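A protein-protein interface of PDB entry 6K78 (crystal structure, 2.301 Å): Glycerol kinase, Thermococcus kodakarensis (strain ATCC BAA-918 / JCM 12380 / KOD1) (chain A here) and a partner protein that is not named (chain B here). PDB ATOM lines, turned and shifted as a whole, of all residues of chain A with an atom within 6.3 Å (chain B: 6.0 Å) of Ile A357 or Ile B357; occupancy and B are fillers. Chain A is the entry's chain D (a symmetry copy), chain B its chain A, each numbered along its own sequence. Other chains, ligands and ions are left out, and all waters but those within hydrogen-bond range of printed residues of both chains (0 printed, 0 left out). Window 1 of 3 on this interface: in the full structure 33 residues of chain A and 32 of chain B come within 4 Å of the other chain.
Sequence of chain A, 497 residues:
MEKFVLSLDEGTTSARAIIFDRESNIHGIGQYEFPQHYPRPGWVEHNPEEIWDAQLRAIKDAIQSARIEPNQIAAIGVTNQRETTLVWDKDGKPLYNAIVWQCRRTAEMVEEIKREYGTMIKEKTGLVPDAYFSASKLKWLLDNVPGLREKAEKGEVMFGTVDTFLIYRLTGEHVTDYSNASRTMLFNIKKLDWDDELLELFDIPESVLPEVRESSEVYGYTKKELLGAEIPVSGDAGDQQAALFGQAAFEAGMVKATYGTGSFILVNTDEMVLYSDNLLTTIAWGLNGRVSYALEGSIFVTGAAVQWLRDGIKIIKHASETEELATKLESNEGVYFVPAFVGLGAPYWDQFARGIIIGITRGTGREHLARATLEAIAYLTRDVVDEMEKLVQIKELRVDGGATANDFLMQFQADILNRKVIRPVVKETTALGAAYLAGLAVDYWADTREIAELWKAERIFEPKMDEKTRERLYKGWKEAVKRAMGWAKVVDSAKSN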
ATOM      1  N   TRP A 308     -21.848 -21.630  -4.015  1.00  0.00           N
ATOM      2  CA  TRP A 308     -21.175 -21.912  -2.748  1.00  0.00           C
ATOM      3  C   TRP A 308     -20.977 -20.643  -1.937  1.00  0.00           C
ATOM      4  O   TRP A 308     -21.088 -20.662  -0.710  1.00  0.00           O
ATOM      5  CB  TRP A 308     -19.826 -22.595  -2.988  1.00  0.00           C
ATOM      6  CG  TRP A 308     -19.052 -22.853  -1.706  1.00  0.00           C
ATOM      7  CD1 TRP A 308     -19.299 -23.829  -0.783  1.00  0.00           C
ATOM      8  CD2 TRP A 308     -17.915 -22.123  -1.219  1.00  0.00           C
ATOM      9  NE1 TRP A 308     -18.396 -23.747   0.252  1.00  0.00           N
ATOM     10  CE2 TRP A 308     -17.535 -22.709   0.009  1.00  0.00           C
ATOM     11  CE3 TRP A 308     -17.190 -21.024  -1.694  1.00  0.00           C
ATOM     12  CZ2 TRP A 308     -16.463 -22.229   0.771  1.00  0.00           C
ATOM     13  CZ3 TRP A 308     -16.116 -20.552  -0.934  1.00  0.00           C
ATOM     14  CH2 TRP A 308     -15.765 -21.152   0.279  1.00  0.00           C
ATOM     15  N   ILE A 313     -20.833 -20.833   2.395  1.00  0.00           N
ATOM     16  CA  ILE A 313     -20.404 -19.953   3.467  1.00  0.00           C
ATOM     17  C   ILE A 313     -21.307 -18.737   3.621  1.00  0.00           C
ATOM     18  O   ILE A 313     -21.104 -17.939   4.538  1.00  0.00           O
ATOM     19  CB  ILE A 313     -18.932 -19.543   3.285  1.00  0.00           C
ATOM     20  CG1 ILE A 313     -18.678 -18.985   1.886  1.00  0.00           C
ATOM     21  CG2 ILE A 313     -18.017 -20.734   3.598  1.00  0.00           C
ATOM     22  CD1 ILE A 313     -17.433 -18.164   1.850  1.00  0.00           C
ATOM     23  N   VAL A 335      -5.434 -12.315  -4.132  1.00  0.00           N
ATOM     24  CA  VAL A 335      -6.328 -13.377  -3.688  1.00  0.00           C
ATOM     25  C   VAL A 335      -6.853 -14.123  -4.901  1.00  0.00           C
ATOM     26  O   VAL A 335      -7.466 -13.521  -5.786  1.00  0.00           O
ATOM     27  CB  VAL A 335      -7.491 -12.806  -2.867  1.00  0.00           C
ATOM     28  CG1 VAL A 335      -8.447 -13.923  -2.466  1.00  0.00           C
ATOM     29  CG2 VAL A 335      -6.960 -12.040  -1.655  1.00  0.00           C
ATOM     30  N   TYR A 336      -6.637 -15.434  -4.931  1.00  0.00           N
ATOM     31  CA  TYR A 336      -7.181 -16.288  -5.968  1.00  0.00           C
ATOM     32  C   TYR A 336      -7.990 -17.405  -5.328  1.00  0.00           C
ATOM     33  O   TYR A 336      -7.724 -17.821  -4.198  1.00  0.00           O
ATOM     34  CB  TYR A 336      -6.075 -16.900  -6.852  1.00  0.00           C
ATOM     35  CG  TYR A 336      -5.426 -15.912  -7.810  1.00  0.00           C
ATOM     36  CD1 TYR A 336      -4.636 -14.880  -7.333  1.00  0.00           C
ATOM     37  CD2 TYR A 336      -5.598 -16.025  -9.194  1.00  0.00           C
ATOM     38  CE1 TYR A 336      -4.039 -13.972  -8.191  1.00  0.00           C
ATOM     39  CE2 TYR A 336      -5.016 -15.115 -10.060  1.00  0.00           C
ATOM     40  CZ  TYR A 336      -4.229 -14.094  -9.548  1.00  0.00           C
ATOM     41  OH  TYR A 336      -3.627 -13.181 -10.382  1.00  0.00           O
ATOM     42  N   PHE A 337      -8.942 -17.935  -6.091  1.00  0.00           N
ATOM     43  CA  PHE A 337      -9.829 -18.999  -5.631  1.00  0.00           C
ATOM     44  C   PHE A 337      -9.936 -20.034  -6.737  1.00  0.00           C
ATOM     45  O   PHE A 337     -10.494 -19.734  -7.791  1.00  0.00           O
ATOM     46  CB  PHE A 337     -11.208 -18.427  -5.297  1.00  0.00           C
ATOM     47  CG  PHE A 337     -12.231 -19.440  -4.895  1.00  0.00           C
ATOM     48  CD1 PHE A 337     -11.871 -20.703  -4.427  1.00  0.00           C
ATOM     49  CD2 PHE A 337     -13.577 -19.109  -4.962  1.00  0.00           C
ATOM     50  CE1 PHE A 337     -12.827 -21.610  -4.037  1.00  0.00           C
ATOM     51  CE2 PHE A 337     -14.556 -20.018  -4.573  1.00  0.00           C
ATOM     52  CZ  PHE A 337     -14.174 -21.276  -4.099  1.00  0.00           C
ATOM     53  N   VAL A 338      -9.451 -21.251  -6.483  1.00  0.00           N
ATOM     54  CA  VAL A 338      -9.557 -22.352  -7.433  1.00  0.00           C
ATOM     55  C   VAL A 338     -10.665 -23.295  -6.974  1.00  0.00           C
ATOM     56  O   VAL A 338     -10.431 -24.160  -6.120  1.00  0.00           O
ATOM     57  CB  VAL A 338      -8.203 -23.070  -7.592  1.00  0.00           C
ATOM     58  CG1 VAL A 338      -8.318 -24.274  -8.525  1.00  0.00           C
ATOM     59  CG2 VAL A 338      -7.148 -22.101  -8.088  1.00  0.00           C
ATOM     60  N   GLY A 355     -10.647 -27.444  -3.469  1.00  0.00           N
ATOM     61  CA  GLY A 355     -10.741 -26.002  -3.539  1.00  0.00           C
ATOM     62  C   GLY A 355      -9.660 -25.336  -2.708  1.00  0.00           C
ATOM     63  O   GLY A 355      -9.313 -25.793  -1.621  1.00  0.00           O
ATOM     64  N   ILE A 356      -9.126 -24.238  -3.231  1.00  0.00           N
ATOM     65  CA  ILE A 356      -8.142 -23.449  -2.504  1.00  0.00           C
ATOM     66  C   ILE A 356      -8.486 -21.968  -2.659  1.00  0.00           C
ATOM     67  O   ILE A 356      -8.878 -21.520  -3.740  1.00  0.00           O
ATOM     68  CB  ILE A 356      -6.718 -23.761  -3.005  1.00  0.00           C
ATOM     69  CG1 ILE A 356      -5.670 -23.075  -2.146  1.00  0.00           C
ATOM     70  CG2 ILE A 356      -6.534 -23.326  -4.449  1.00  0.00           C
ATOM     71  CD1 ILE A 356      -4.282 -23.133  -2.770  1.00  0.00           C
ATOM     72  N   ILE A 357      -8.385 -21.223  -1.561  1.00  0.00           N
ATOM     73  CA  ILE A 357      -8.382 -19.760  -1.552  1.00  0.00           C
ATOM     74  C   ILE A 357      -7.027 -19.336  -1.020  1.00  0.00           C
ATOM     75  O   ILE A 357      -6.626 -19.762   0.072  1.00  0.00           O
ATOM     76  CB  ILE A 357      -9.495 -19.177  -0.653  1.00  0.00           C
ATOM     77  CG1 ILE A 357     -10.901 -19.671  -1.046  1.00  0.00           C
ATOM     78  CG2 ILE A 357      -9.405 -17.651  -0.608  1.00  0.00           C
ATOM     79  CD1 ILE A 357     -12.014 -19.173  -0.059  1.00  0.00           C
ATOM     80  N   ILE A 358      -6.312 -18.501  -1.770  1.00  0.00           N
ATOM     81  CA  ILE A 358      -4.947 -18.185  -1.387  1.00  0.00           C
ATOM     82  C   ILE A 358      -4.684 -16.701  -1.550  1.00  0.00           C
ATOM     83  O   ILE A 358      -5.312 -16.020  -2.367  1.00  0.00           O
ATOM     84  CB  ILE A 358      -3.946 -19.016  -2.190  1.00  0.00           C
ATOM     85  CG1 ILE A 358      -2.537 -18.859  -1.598  1.00  0.00           C
ATOM     86  CG2 ILE A 358      -4.026 -18.634  -3.672  1.00  0.00           C
ATOM     87  CD1 ILE A 358      -1.602 -20.011  -1.958  1.00  0.00           C
ATOM     88  N   GLY A 359      -3.747 -16.197  -0.744  1.00  0.00           N
ATOM     89  CA  GLY A 359      -3.473 -14.782  -0.668  1.00  0.00           C
ATOM     90  C   GLY A 359      -4.144 -14.090   0.487  1.00  0.00           C
ATOM     91  O   GLY A 359      -4.146 -12.853   0.527  1.00  0.00           O
ATOM     92  N   ILE A 360      -4.706 -14.848   1.432  1.00  0.00           N
ATOM     93  CA  ILE A 360      -5.461 -14.255   2.522  1.00  0.00           C
ATOM     94  C   ILE A 360      -4.515 -13.506   3.454  1.00  0.00           C
ATOM     95  O   ILE A 360      -3.500 -14.043   3.906  1.00  0.00           O
ATOM     96  CB  ILE A 360      -6.262 -15.329   3.270  1.00  0.00           C
ATOM     97  CG1 ILE A 360      -7.140 -16.104   2.306  1.00  0.00           C
ATOM     98  CG2 ILE A 360      -7.111 -14.691   4.354  1.00  0.00           C
ATOM     99  CD1 ILE A 360      -7.615 -17.423   2.828  1.00  0.00           C
ATOM    100  N   LEU A 369     -13.269 -12.317  -2.052  1.00  0.00           N
ATOM    101  CA  LEU A 369     -13.795 -13.646  -2.345  1.00  0.00           C
ATOM    102  C   LEU A 369     -14.770 -13.590  -3.514  1.00  0.00           C
ATOM    103  O   LEU A 369     -14.751 -14.465  -4.379  1.00  0.00           O
ATOM    104  CB  LEU A 369     -14.468 -14.252  -1.119  1.00  0.00           C
ATOM    105  CG  LEU A 369     -13.652 -15.223  -0.266  1.00  0.00           C
ATOM    106  CD1 LEU A 369     -12.361 -14.565   0.189  1.00  0.00           C
ATOM    107  CD2 LEU A 369     -14.464 -15.710   0.956  1.00  0.00           C
ATOM    108  N   ALA A 372     -12.497 -12.963  -6.637  1.00  0.00           N
ATOM    109  CA  ALA A 372     -11.726 -14.154  -6.957  1.00  0.00           C
ATOM    110  C   ALA A 372     -12.598 -15.253  -7.535  1.00  0.00           C
ATOM    111  O   ALA A 372     -12.133 -16.033  -8.373  1.00  0.00           O
ATOM    112  CB  ALA A 372     -10.991 -14.663  -5.714  1.00  0.00           C
ATOM    113  N   TRP B 308     -10.376 -12.223  11.843  1.00  0.00           N
ATOM    114  CA  TRP B 308     -10.611 -12.194  10.404  1.00  0.00           C
ATOM    115  C   TRP B 308     -11.910 -12.912  10.021  1.00  0.00           C
ATOM    116  O   TRP B 308     -12.622 -12.464   9.114  1.00  0.00           O
ATOM    117  CB  TRP B 308      -9.421 -12.796   9.657  1.00  0.00           C
ATOM    118  CG  TRP B 308      -9.674 -12.897   8.181  1.00  0.00           C
ATOM    119  CD1 TRP B 308      -9.608 -11.882   7.265  1.00  0.00           C
ATOM    120  CD2 TRP B 308     -10.069 -14.068   7.456  1.00  0.00           C
ATOM    121  NE1 TRP B 308      -9.923 -12.356   6.009  1.00  0.00           N
ATOM    122  CE2 TRP B 308     -10.209 -13.693   6.098  1.00  0.00           C
ATOM    123  CE3 TRP B 308     -10.321 -15.395   7.823  1.00  0.00           C
ATOM    124  CZ2 TRP B 308     -10.587 -14.598   5.107  1.00  0.00           C
ATOM    125  CZ3 TRP B 308     -10.677 -16.296   6.840  1.00  0.00           C
ATOM    126  CH2 TRP B 308     -10.814 -15.893   5.496  1.00  0.00           C
ATOM    127  N   ILE B 313     -14.335 -11.794   6.294  1.00  0.00           N
ATOM    128  CA  ILE B 313     -15.437 -12.419   5.575  1.00  0.00           C
ATOM    129  C   ILE B 313     -16.722 -12.454   6.391  1.00  0.00           C
ATOM    130  O   ILE B 313     -17.780 -12.797   5.839  1.00  0.00           O
ATOM    131  CB  ILE B 313     -15.077 -13.855   5.142  1.00  0.00           C
ATOM    132  CG1 ILE B 313     -14.597 -14.696   6.323  1.00  0.00           C
ATOM    133  CG2 ILE B 313     -14.017 -13.835   4.063  1.00  0.00           C
ATOM    134  CD1 ILE B 313     -14.394 -16.167   5.949  1.00  0.00           C
ATOM    135  N   VAL B 335     -10.534 -29.841   5.456  1.00  0.00           N
ATOM    136  CA  VAL B 335     -10.408 -28.393   5.348  1.00  0.00           C
ATOM    137  C   VAL B 335      -9.362 -27.894   6.337  1.00  0.00           C
ATOM    138  O   VAL B 335      -9.446 -28.156   7.545  1.00  0.00           O
ATOM    139  CB  VAL B 335     -11.755 -27.695   5.575  1.00  0.00           C
ATOM    140  CG1 VAL B 335     -11.536 -26.194   5.625  1.00  0.00           C
ATOM    141  CG2 VAL B 335     -12.732 -28.072   4.470  1.00  0.00           C
ATOM    142  N   TYR B 336      -8.386 -27.156   5.817  1.00  0.00           N
ATOM    143  CA  TYR B 336      -7.344 -26.527   6.604  1.00  0.00           C
ATOM    144  C   TYR B 336      -7.297 -25.048   6.250  1.00  0.00           C
ATOM    145  O   TYR B 336      -7.694 -24.634   5.158  1.00  0.00           O
ATOM    146  CB  TYR B 336      -5.970 -27.184   6.357  1.00  0.00           C
ATOM    147  CG  TYR B 336      -5.802 -28.538   7.029  1.00  0.00           C
ATOM    148  CD1 TYR B 336      -6.514 -29.656   6.582  1.00  0.00           C
ATOM    149  CD2 TYR B 336      -4.959 -28.698   8.129  1.00  0.00           C
ATOM    150  CE1 TYR B 336      -6.379 -30.895   7.195  1.00  0.00           C
ATOM    151  CE2 TYR B 336      -4.823 -29.948   8.755  1.00  0.00           C
ATOM    152  CZ  TYR B 336      -5.524 -31.027   8.280  1.00  0.00           C
ATOM    153  OH  TYR B 336      -5.396 -32.249   8.881  1.00  0.00           O
ATOM    154  N   PHE B 337      -6.825 -24.261   7.202  1.00  0.00           N
ATOM    155  CA  PHE B 337      -6.682 -22.825   7.055  1.00  0.00           C
ATOM    156  C   PHE B 337      -5.330 -22.480   7.667  1.00  0.00           C
ATOM    157  O   PHE B 337      -5.136 -22.686   8.867  1.00  0.00           O
ATOM    158  CB  PHE B 337      -7.836 -22.091   7.767  1.00  0.00           C
ATOM    159  CG  PHE B 337      -7.742 -20.571   7.735  1.00  0.00           C
ATOM    160  CD1 PHE B 337      -6.900 -19.904   6.851  1.00  0.00           C
ATOM    161  CD2 PHE B 337      -8.515 -19.818   8.611  1.00  0.00           C
ATOM    162  CE1 PHE B 337      -6.831 -18.525   6.837  1.00  0.00           C
ATOM    163  CE2 PHE B 337      -8.456 -18.444   8.615  1.00  0.00           C
ATOM    164  CZ  PHE B 337      -7.606 -17.786   7.712  1.00  0.00           C
ATOM    165  N   VAL B 338      -4.389 -22.003   6.851  1.00  0.00           N
ATOM    166  CA  VAL B 338      -3.114 -21.541   7.383  1.00  0.00           C
ATOM    167  C   VAL B 338      -3.172 -20.024   7.414  1.00  0.00           C
ATOM    168  O   VAL B 338      -3.004 -19.376   6.369  1.00  0.00           O
ATOM    169  CB  VAL B 338      -1.916 -22.039   6.560  1.00  0.00           C
ATOM    170  CG1 VAL B 338      -0.640 -21.538   7.197  1.00  0.00           C
ATOM    171  CG2 VAL B 338      -1.882 -23.537   6.523  1.00  0.00           C
ATOM    172  N   GLY B 355      -1.885 -16.370   3.540  1.00  0.00           N
ATOM    173  CA  GLY B 355      -2.944 -17.216   4.057  1.00  0.00           C
ATOM    174  C   GLY B 355      -3.576 -18.055   2.964  1.00  0.00           C
ATOM    175  O   GLY B 355      -3.753 -17.603   1.828  1.00  0.00           O
ATOM    176  N   ILE B 356      -3.928 -19.288   3.321  1.00  0.00           N
ATOM    177  CA  ILE B 356      -4.553 -20.240   2.418  1.00  0.00           C
ATOM    178  C   ILE B 356      -5.645 -21.019   3.160  1.00  0.00           C
ATOM    179  O   ILE B 356      -5.467 -21.411   4.321  1.00  0.00           O
ATOM    180  CB  ILE B 356      -3.489 -21.194   1.829  1.00  0.00           C
ATOM    181  CG1 ILE B 356      -4.115 -22.211   0.887  1.00  0.00           C
ATOM    182  CG2 ILE B 356      -2.726 -21.921   2.922  1.00  0.00           C
ATOM    183  CD1 ILE B 356      -3.129 -23.316   0.465  1.00  0.00           C
ATOM    184  N   ILE B 357      -6.784 -21.231   2.485  1.00  0.00           N
ATOM    185  CA  ILE B 357      -7.793 -22.222   2.851  1.00  0.00           C
ATOM    186  C   ILE B 357      -7.825 -23.270   1.748  1.00  0.00           C
ATOM    187  O   ILE B 357      -7.993 -22.919   0.573  1.00  0.00           O
ATOM    188  CB  ILE B 357      -9.195 -21.602   3.015  1.00  0.00           C
ATOM    189  CG1 ILE B 357      -9.214 -20.466   4.037  1.00  0.00           C
ATOM    190  CG2 ILE B 357     -10.233 -22.688   3.369  1.00  0.00           C
ATOM    191  CD1 ILE B 357     -10.566 -19.797   4.100  1.00  0.00           C
ATOM    192  N   ILE B 358      -7.728 -24.555   2.124  1.00  0.00           N
ATOM    193  CA  ILE B 358      -7.599 -25.650   1.171  1.00  0.00           C
ATOM    194  C   ILE B 358      -8.461 -26.827   1.614  1.00  0.00           C
ATOM    195  O   ILE B 358      -8.680 -27.050   2.806  1.00  0.00           O
ATOM    196  CB  ILE B 358      -6.130 -26.091   1.006  1.00  0.00           C
ATOM    197  CG1 ILE B 358      -6.000 -27.098  -0.137  1.00  0.00           C
ATOM    198  CG2 ILE B 358      -5.610 -26.738   2.279  1.00  0.00           C
ATOM    199  CD1 ILE B 358      -4.562 -27.463  -0.473  1.00  0.00           C
ATOM    200  N   GLY B 359      -8.934 -27.595   0.640  1.00  0.00           N
ATOM    201  CA  GLY B 359      -9.877 -28.661   0.872  1.00  0.00           C
ATOM    202  C   GLY B 359     -11.312 -28.296   0.586  1.00  0.00           C
ATOM    203  O   GLY B 359     -12.213 -29.054   0.960  1.00  0.00           O
ATOM    204  N   ILE B 360     -11.564 -27.156  -0.056  1.00  0.00           N
ATOM    205  CA  ILE B 360     -12.939 -26.697  -0.201  1.00  0.00           C
ATOM    206  C   ILE B 360     -13.670 -27.577  -1.204  1.00  0.00           C
ATOM    207  O   ILE B 360     -13.115 -27.991  -2.234  1.00  0.00           O
ATOM    208  CB  ILE B 360     -12.982 -25.214  -0.615  1.00  0.00           C
ATOM    209  CG1 ILE B 360     -12.271 -24.354   0.423  1.00  0.00           C
ATOM    210  CG2 ILE B 360     -14.408 -24.739  -0.791  1.00  0.00           C
ATOM    211  CD1 ILE B 360     -11.904 -22.998  -0.082  1.00  0.00           C
ATOM    212  N   LEU B 369     -14.921 -23.705   8.218  1.00  0.00           N
ATOM    213  CA  LEU B 369     -13.990 -22.595   8.349  1.00  0.00           C
ATOM    214  C   LEU B 369     -13.690 -22.302   9.815  1.00  0.00           C
ATOM    215  O   LEU B 369     -12.546 -21.989  10.169  1.00  0.00           O
ATOM    216  CB  LEU B 369     -14.545 -21.350   7.641  1.00  0.00           C
ATOM    217  CG  LEU B 369     -14.052 -21.108   6.213  1.00  0.00           C
ATOM    218  CD1 LEU B 369     -13.990 -22.401   5.433  1.00  0.00           C
ATOM    219  CD2 LEU B 369     -14.914 -20.092   5.465  1.00  0.00           C
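The backbone NH of Gly A359 sits at hydrogen-bond distance from the backbone carbonyl oxygen of Gly B355.
The backbone NH of Gly B355 lies within hydrogen-bond range of the backbone carbonyl oxygen of Ile A360, 2.9 Å away.
The backbone NH (N) of Ile A357 sits at hydrogen-bond distance from the backbone carbonyl oxygen (O) of Ile B357, at 2.8 Å.
N of Gly B359 sits at hydrogen-bond distance from O of Gly A355 (2.9 Å).
The backbone carbonyl oxygen (O) of Ile B360 is in hydrogen-bond range of the backbone NH (N) of Gly A355.
O of Trp B308 sits at hydrogen-bond distance from N of Ile B313 (3.4 Å).
N of Tyr B336 is in hydrogen-bond range of O of Ile B358, at 3.0 Å.
O of Ile B356 sits at hydrogen-bond distance from N of Val B338 (2.8 Å).
The backbone NH of Ile A313 sits at hydrogen-bond distance from the backbone carbonyl oxygen of Trp A308.
N of Ile A358 lies within hydrogen-bond range of O of Tyr A336.
The backbone NH (N) of Val A338 is in hydrogen-bond range of the backbone carbonyl oxygen (O) of Ile A356 (2.8 Å).
Among the printed residues, pairs that only touch across the chains: Trp A308 with Ile B360 (3.6 Å), Ile A313 with Leu B369 (3.7 Å), Gly A355 with Ile B357 (3.8 Å), Gly A355 with Ile B358 (3.3 Å), Ile A356 with Ile B356 (3.4 Å), Ile A356 with Ile B357 (3.1 Å), Ile A357 with Gly B355 (3.9999 Å), Ile A357 with Ile B356 (3.2 Å), Ile A357 with Ile B360 (3.6 Å), Ile A358 with Gly B355 (3.5 Å), Ile A360 with Trp B308 (3.6 Å), Ile A360 with Ile B357 (3.6 Å) and Leu A369 with Ile B313 (3.7 Å).
Of the printed residues of chain B, Gly A355 touches Ile B357, Ile B358, Gly B359 and Ile B360.
Printed residues of chain B within 4 Å of Ile A357: Gly B355, Ile B356, Ile B357 and Ile B360.
Of the printed residues of chain A, Trp B308 touches Ile A360 (3.6 Å).
Phe B337 touches none of the printed residues of chain A.
Printed residues of chain A within 4 Å of Ile B356: Ile A356 (3.4 Å) and Ile A357 (3.2 Å).
Printed residues of chain A within 4 Å of Ile B357: Gly A355, Ile A356, Ile A357 and Ile A360.
Of the printed residues of chain A, Leu B369 touches Ile A313 (3.7 Å).
The nearest printed residue of chain B that does not touch Ile A357 is Ile B358 (5.0 Å).
Of the 13 printed residues of chain B, 9 touch a printed residue of chain A.
Of the 14 printed residues of chain A, 9 touch a printed residue of chain B.
Hydrophobic or aromatic side chains of chain A within 4 Å of the printed part of chain B: Trp A308, Ile A313, Ile A356, Ile A357, Ile A358, Ile A360 and Leu A369.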
